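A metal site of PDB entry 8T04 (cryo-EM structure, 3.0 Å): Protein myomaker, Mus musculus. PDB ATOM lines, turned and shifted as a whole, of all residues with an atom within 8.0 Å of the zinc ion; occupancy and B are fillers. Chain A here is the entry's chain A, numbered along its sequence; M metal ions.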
ATOM      1  N   PRO A  11      29.011   1.779  14.675  1.00  0.00           N
ATOM      2  CA  PRO A  11      27.676   1.397  14.198  1.00  0.00           C
ATOM      3  C   PRO A  11      27.631   0.721  12.814  1.00  0.00           C
ATOM      4  O   PRO A  11      26.734  -0.083  12.619  1.00  0.00           O
ATOM      5  CB  PRO A  11      26.909   2.726  14.162  1.00  0.00           C
ATOM      6  CG  PRO A  11      27.595   3.562  15.201  1.00  0.00           C
ATOM      7  CD  PRO A  11      29.068   3.205  15.039  1.00  0.00           C
ATOM      8  N   THR A  12      28.554   1.031  11.904  1.00  0.00           N
ATOM      9  CA  THR A  12      28.653   0.361  10.579  1.00  0.00           C
ATOM     10  C   THR A  12      29.173  -1.061  10.759  1.00  0.00           C
ATOM     11  O   THR A  12      28.485  -1.994  10.316  1.00  0.00           O
ATOM     12  CB  THR A  12      29.529   1.127   9.570  1.00  0.00           C
ATOM     13  OG1 THR A  12      29.042   2.467   9.472  1.00  0.00           O
ATOM     14  CG2 THR A  12      29.515   0.471   8.204  1.00  0.00           C
ATOM     15  N   SER A  14      29.761  -3.036  13.503  1.00  0.00           N
ATOM     16  CA  SER A  14      29.061  -3.889  14.491  1.00  0.00           C
ATOM     17  C   SER A  14      27.738  -4.432  13.937  1.00  0.00           C
ATOM     18  O   SER A  14      27.206  -5.374  14.560  1.00  0.00           O
ATOM     19  CB  SER A  14      28.827  -3.171  15.791  1.00  0.00           C
ATOM     20  OG  SER A  14      28.006  -2.030  15.599  1.00  0.00           O
ATOM     21  N   SER A  15      27.213  -3.884  12.832  1.00  0.00           N
ATOM     22  CA  SER A  15      26.058  -4.455  12.081  1.00  0.00           C
ATOM     23  C   SER A  15      26.400  -5.854  11.539  1.00  0.00           C
ATOM     24  O   SER A  15      25.452  -6.595  11.251  1.00  0.00           O
ATOM     25  CB  SER A  15      25.589  -3.547  10.973  1.00  0.00           C
ATOM     26  OG  SER A  15      26.514  -3.542   9.896  1.00  0.00           O
ATOM     27  N   PHE A  18      25.045  -9.504  12.865  1.00  0.00           N
ATOM     28  CA  PHE A  18      23.935 -10.266  12.233  1.00  0.00           C
ATOM     29  C   PHE A  18      24.472 -11.365  11.300  1.00  0.00           C
ATOM     30  O   PHE A  18      23.646 -12.219  10.917  1.00  0.00           O
ATOM     31  CB  PHE A  18      22.965  -9.334  11.493  1.00  0.00           C
ATOM     32  CG  PHE A  18      22.242  -8.358  12.384  1.00  0.00           C
ATOM     33  CD1 PHE A  18      21.343  -8.795  13.339  1.00  0.00           C
ATOM     34  CD2 PHE A  18      22.465  -6.995  12.261  1.00  0.00           C
ATOM     35  CE1 PHE A  18      20.684  -7.892  14.167  1.00  0.00           C
ATOM     36  CE2 PHE A  18      21.792  -6.092  13.084  1.00  0.00           C
ATOM     37  CZ  PHE A  18      20.911  -6.541  14.033  1.00  0.00           C
ATOM     38  N   THR A  40      18.229  -7.658   6.482  1.00  0.00           N
ATOM     39  CA  THR A  40      18.386  -6.727   7.633  1.00  0.00           C
ATOM     40  C   THR A  40      19.840  -6.261   7.727  1.00  0.00           C
ATOM     41  O   THR A  40      20.064  -5.044   7.737  1.00  0.00           O
ATOM     42  CB  THR A  40      17.921  -7.364   8.949  1.00  0.00           C
ATOM     43  OG1 THR A  40      16.559  -7.755   8.788  1.00  0.00           O
ATOM     44  CG2 THR A  40      18.061  -6.447  10.141  1.00  0.00           C
ATOM     45  N   PHE A  43      20.844  -3.829   4.858  1.00  0.00           N
ATOM     46  CA  PHE A  43      20.171  -2.515   4.926  1.00  0.00           C
ATOM     47  C   PHE A  43      20.576  -1.758   6.208  1.00  0.00           C
ATOM     48  O   PHE A  43      20.651  -0.519   6.137  1.00  0.00           O
ATOM     49  CB  PHE A  43      18.655  -2.651   4.761  1.00  0.00           C
ATOM     50  CG  PHE A  43      18.220  -2.718   3.318  1.00  0.00           C
ATOM     51  CD1 PHE A  43      18.263  -1.578   2.520  1.00  0.00           C
ATOM     52  CD2 PHE A  43      17.814  -3.912   2.740  1.00  0.00           C
ATOM     53  CE1 PHE A  43      17.882  -1.636   1.184  1.00  0.00           C
ATOM     54  CE2 PHE A  43      17.447  -3.970   1.409  1.00  0.00           C
ATOM     55  CZ  PHE A  43      17.475  -2.827   0.628  1.00  0.00           C
ATOM     56  N   VAL A  44      20.833  -2.467   7.319  1.00  0.00           N
ATOM     57  CA  VAL A  44      21.334  -1.841   8.585  1.00  0.00           C
ATOM     58  C   VAL A  44      22.773  -1.363   8.369  1.00  0.00           C
ATOM     59  O   VAL A  44      23.062  -0.215   8.751  1.00  0.00           O
ATOM     60  CB  VAL A  44      21.185  -2.800   9.790  1.00  0.00           C
ATOM     61  CG1 VAL A  44      21.949  -2.310  11.025  1.00  0.00           C
ATOM     62  CG2 VAL A  44      19.720  -3.005  10.153  1.00  0.00           C
ATOM     63  N   ALA A  45      23.633  -2.201   7.778  1.00  0.00           N
ATOM     64  CA  ALA A  45      25.057  -1.875   7.463  1.00  0.00           C
ATOM     65  C   ALA A  45      25.126  -0.626   6.590  1.00  0.00           C
ATOM     66  O   ALA A  45      25.911   0.286   6.930  1.00  0.00           O
ATOM     67  CB  ALA A  45      25.735  -3.043   6.793  1.00  0.00           C
ATOM     68  N   SER A  47      22.616   1.577   5.932  1.00  0.00           N
ATOM     69  CA  SER A  47      21.919   2.699   6.625  1.00  0.00           C
ATOM     70  C   SER A  47      22.930   3.494   7.458  1.00  0.00           C
ATOM     71  O   SER A  47      22.859   4.748   7.423  1.00  0.00           O
ATOM     72  CB  SER A  47      20.766   2.227   7.471  1.00  0.00           C
ATOM     73  OG  SER A  47      20.138   3.319   8.127  1.00  0.00           O
ATOM     74  N   HIS A  48      23.824   2.807   8.174  1.00  0.00           N
ATOM     75  CA  HIS A  48      24.859   3.423   9.046  1.00  0.00           C
ATOM     76  C   HIS A  48      26.014   3.986   8.201  1.00  0.00           C
ATOM     77  O   HIS A  48      26.484   5.093   8.533  1.00  0.00           O
ATOM     78  CB  HIS A  48      25.354   2.437  10.107  1.00  0.00           C
ATOM     79  CG  HIS A  48      24.308   2.090  11.125  1.00  0.00           C
ATOM     80  ND1 HIS A  48      23.682   3.062  11.879  1.00  0.00           N
ATOM     81  CD2 HIS A  48      23.788   0.904  11.506  1.00  0.00           C
ATOM     82  CE1 HIS A  48      22.813   2.482  12.683  1.00  0.00           C
ATOM     83  NE2 HIS A  48      22.863   1.158  12.472  1.00  0.00           N
ATOM     84  N   SER A  70      16.128  -0.656   6.779  1.00  0.00           N
ATOM     85  CA  SER A  70      16.841  -0.851   8.078  1.00  0.00           C
ATOM     86  C   SER A  70      15.809  -1.159   9.173  1.00  0.00           C
ATOM     87  O   SER A  70      15.968  -2.176   9.866  1.00  0.00           O
ATOM     88  CB  SER A  70      17.676   0.352   8.424  1.00  0.00           C
ATOM     89  OG  SER A  70      18.151   0.282   9.765  1.00  0.00           O
ATOM     90  N   THR A  74      14.592  -4.927  10.530  1.00  0.00           N
ATOM     91  CA  THR A  74      14.823  -5.136  11.985  1.00  0.00           C
ATOM     92  C   THR A  74      13.535  -5.642  12.640  1.00  0.00           C
ATOM     93  O   THR A  74      13.611  -6.648  13.366  1.00  0.00           O
ATOM     94  CB  THR A  74      15.320  -3.854  12.680  1.00  0.00           C
ATOM     95  OG1 THR A  74      16.497  -3.412  12.011  1.00  0.00           O
ATOM     96  CG2 THR A  74      15.631  -4.068  14.146  1.00  0.00           C
ATOM     97  N   TYR A 118       8.152  -1.666  16.836  1.00  0.00           N
ATOM     98  CA  TYR A 118       8.860  -2.855  17.383  1.00  0.00           C
ATOM     99  C   TYR A 118       8.014  -3.575  18.451  1.00  0.00           C
ATOM    100  O   TYR A 118       8.084  -4.829  18.486  1.00  0.00           O
ATOM    101  CB  TYR A 118      10.223  -2.483  17.958  1.00  0.00           C
ATOM    102  CG  TYR A 118      11.120  -1.732  17.006  1.00  0.00           C
ATOM    103  CD1 TYR A 118      11.740  -2.359  15.940  1.00  0.00           C
ATOM    104  CD2 TYR A 118      11.346  -0.375  17.166  1.00  0.00           C
ATOM    105  CE1 TYR A 118      12.560  -1.674  15.060  1.00  0.00           C
ATOM    106  CE2 TYR A 118      12.161   0.332  16.296  1.00  0.00           C
ATOM    107  CZ  TYR A 118      12.775  -0.313  15.245  1.00  0.00           C
ATOM    108  OH  TYR A 118      13.584   0.377  14.390  1.00  0.00           O
ATOM    109  N   ARG A 168      18.971   0.306  23.086  1.00  0.00           N
ATOM    110  CA  ARG A 168      18.549   1.134  21.933  1.00  0.00           C
ATOM    111  C   ARG A 168      17.556   2.227  22.382  1.00  0.00           C
ATOM    112  O   ARG A 168      17.709   3.366  21.886  1.00  0.00           O
ATOM    113  CB  ARG A 168      17.958   0.271  20.814  1.00  0.00           C
ATOM    114  CG  ARG A 168      17.903   0.954  19.459  1.00  0.00           C
ATOM    115  CD  ARG A 168      16.500   1.001  18.894  1.00  0.00           C
ATOM    116  NE  ARG A 168      16.435   1.682  17.597  1.00  0.00           N
ATOM    117  CZ  ARG A 168      16.476   1.093  16.397  1.00  0.00           C
ATOM    118  NH1 ARG A 168      16.573  -0.224  16.274  1.00  0.00           N
ATOM    119  NH2 ARG A 168      16.404   1.841  15.303  1.00  0.00           N
ATOM    120  N   GLU A 172      20.858   4.741  24.866  1.00  0.00           N
ATOM    121  CA  GLU A 172      21.497   5.210  23.603  1.00  0.00           C
ATOM    122  C   GLU A 172      21.817   6.708  23.655  1.00  0.00           C
ATOM    123  O   GLU A 172      22.758   7.133  22.945  1.00  0.00           O
ATOM    124  CB  GLU A 172      20.597   4.887  22.408  1.00  0.00           C
ATOM    125  CG  GLU A 172      21.278   5.029  21.060  1.00  0.00           C
ATOM    126  CD  GLU A 172      20.437   4.543  19.900  1.00  0.00           C
ATOM    127  OE1 GLU A 172      19.807   5.396  19.222  1.00  0.00           O
ATOM    128  OE2 GLU A 172      20.414   3.313  19.667  1.00  0.00           O
ATOM    129  N   TYR A 176      25.637   7.265  21.504  1.00  0.00           N
ATOM    130  CA  TYR A 176      25.047   6.493  20.387  1.00  0.00           C
ATOM    131  C   TYR A 176      26.087   5.520  19.799  1.00  0.00           C
ATOM    132  O   TYR A 176      25.719   4.354  19.550  1.00  0.00           O
ATOM    133  CB  TYR A 176      24.534   7.459  19.314  1.00  0.00           C
ATOM    134  CG  TYR A 176      23.944   6.813  18.076  1.00  0.00           C
ATOM    135  CD1 TYR A 176      24.749   6.454  17.006  1.00  0.00           C
ATOM    136  CD2 TYR A 176      22.582   6.572  17.977  1.00  0.00           C
ATOM    137  CE1 TYR A 176      24.218   5.857  15.870  1.00  0.00           C
ATOM    138  CE2 TYR A 176      22.032   5.977  16.848  1.00  0.00           C
ATOM    139  CZ  TYR A 176      22.854   5.619  15.793  1.00  0.00           C
ATOM    140  OH  TYR A 176      22.313   5.046  14.680  1.00  0.00           O
ATOM    141  N   HIS A 180      24.679   1.921  20.545  1.00  0.00           N
ATOM    142  CA  HIS A 180      24.019   1.383  19.315  1.00  0.00           C
ATOM    143  C   HIS A 180      24.823   0.208  18.745  1.00  0.00           C
ATOM    144  O   HIS A 180      24.194  -0.695  18.167  1.00  0.00           O
ATOM    145  CB  HIS A 180      23.773   2.461  18.251  1.00  0.00           C
ATOM    146  CG  HIS A 180      22.832   2.005  17.184  1.00  0.00           C
ATOM    147  ND1 HIS A 180      21.461   2.032  17.356  1.00  0.00           N
ATOM    148  CD2 HIS A 180      23.045   1.481  15.961  1.00  0.00           C
ATOM    149  CE1 HIS A 180      20.871   1.567  16.275  1.00  0.00           C
ATOM    150  NE2 HIS A 180      21.822   1.213  15.405  1.00  0.00           N
ATOM    151  N   SER A 181      26.158   0.223  18.877  1.00  0.00           N
ATOM    152  CA  SER A 181      27.042  -0.882  18.431  1.00  0.00           C
ATOM    153  C   SER A 181      26.838  -2.120  19.316  1.00  0.00           C
ATOM    154  O   SER A 181      26.959  -3.237  18.784  1.00  0.00           O
ATOM    155  CB  SER A 181      28.488  -0.467  18.359  1.00  0.00           C
ATOM    156  OG  SER A 181      29.049  -0.317  19.656  1.00  0.00           O
ATOM    157  N   TYR A 183      23.895  -2.701  20.846  1.00  0.00           N
ATOM    158  CA  TYR A 183      22.503  -3.065  20.467  1.00  0.00           C
ATOM    159  C   TYR A 183      22.517  -4.098  19.342  1.00  0.00           C
ATOM    160  O   TYR A 183      21.742  -5.078  19.428  1.00  0.00           O
ATOM    161  CB  TYR A 183      21.682  -1.827  20.082  1.00  0.00           C
ATOM    162  CG  TYR A 183      20.479  -2.118  19.205  1.00  0.00           C
ATOM    163  CD1 TYR A 183      19.357  -2.735  19.715  1.00  0.00           C
ATOM    164  CD2 TYR A 183      20.490  -1.793  17.856  1.00  0.00           C
ATOM    165  CE1 TYR A 183      18.248  -3.001  18.927  1.00  0.00           C
ATOM    166  CE2 TYR A 183      19.391  -2.063  17.042  1.00  0.00           C
ATOM    167  CZ  TYR A 183      18.272  -2.677  17.584  1.00  0.00           C
ATOM    168  OH  TYR A 183      17.186  -2.934  16.797  1.00  0.00           O
ATOM    169  N   HIS A 184      23.352  -3.898  18.305  1.00  0.00           N
ATOM    170  CA  HIS A 184      23.535  -4.834  17.166  1.00  0.00           C
ATOM    171  C   HIS A 184      23.981  -6.208  17.686  1.00  0.00           C
ATOM    172  O   HIS A 184      23.434  -7.226  17.215  1.00  0.00           O
ATOM    173  CB  HIS A 184      24.549  -4.303  16.143  1.00  0.00           C
ATOM    174  CG  HIS A 184      24.054  -3.141  15.349  1.00  0.00           C
ATOM    175  ND1 HIS A 184      24.895  -2.153  14.887  1.00  0.00           N
ATOM    176  CD2 HIS A 184      22.810  -2.815  14.930  1.00  0.00           C
ATOM    177  CE1 HIS A 184      24.196  -1.264  14.212  1.00  0.00           C
ATOM    178  NE2 HIS A 184      22.909  -1.646  14.237  1.00  0.00           N
ATOM    179  N   LEU A 187      21.081  -7.816  20.001  1.00  0.00           N
ATOM    180  CA  LEU A 187      19.906  -8.233  19.179  1.00  0.00           C
ATOM    181  C   LEU A 187      20.272  -9.451  18.317  1.00  0.00           C
ATOM    182  O   LEU A 187      19.420 -10.359  18.211  1.00  0.00           O
ATOM    183  CB  LEU A 187      19.416  -7.083  18.296  1.00  0.00           C
ATOM    184  CG  LEU A 187      18.076  -7.329  17.602  1.00  0.00           C
ATOM    185  CD1 LEU A 187      16.926  -7.356  18.612  1.00  0.00           C
ATOM    186  CD2 LEU A 187      17.801  -6.290  16.532  1.00  0.00           C
HETATM  187 ZN    ZN M   1      21.455  -0.016  13.772  1.00  0.00          ZN
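Residues that only touch the zinc ion: Val 44. Within 4 Å of the zinc ion: Val 44, His 48, His 180 and His 184.
The side-chain hydroxyl of Ser 14 lies within hydrogen-bond range of a ring nitrogen (ND1) of His 184. The side-chain carboxylate (OE2) of Glu 172 lies within hydrogen-bond range of a ring nitrogen (ND1) of His 180, 2.8 Å away.
A ring nitrogen (NE2) of His 180 binds the zinc ion, at 2.1 Å. The zinc ion is bound by NE2 of His 184, at 2.2 Å. A ring nitrogen (NE2) of His 48 is bound to the zinc ion (2.2 Å).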
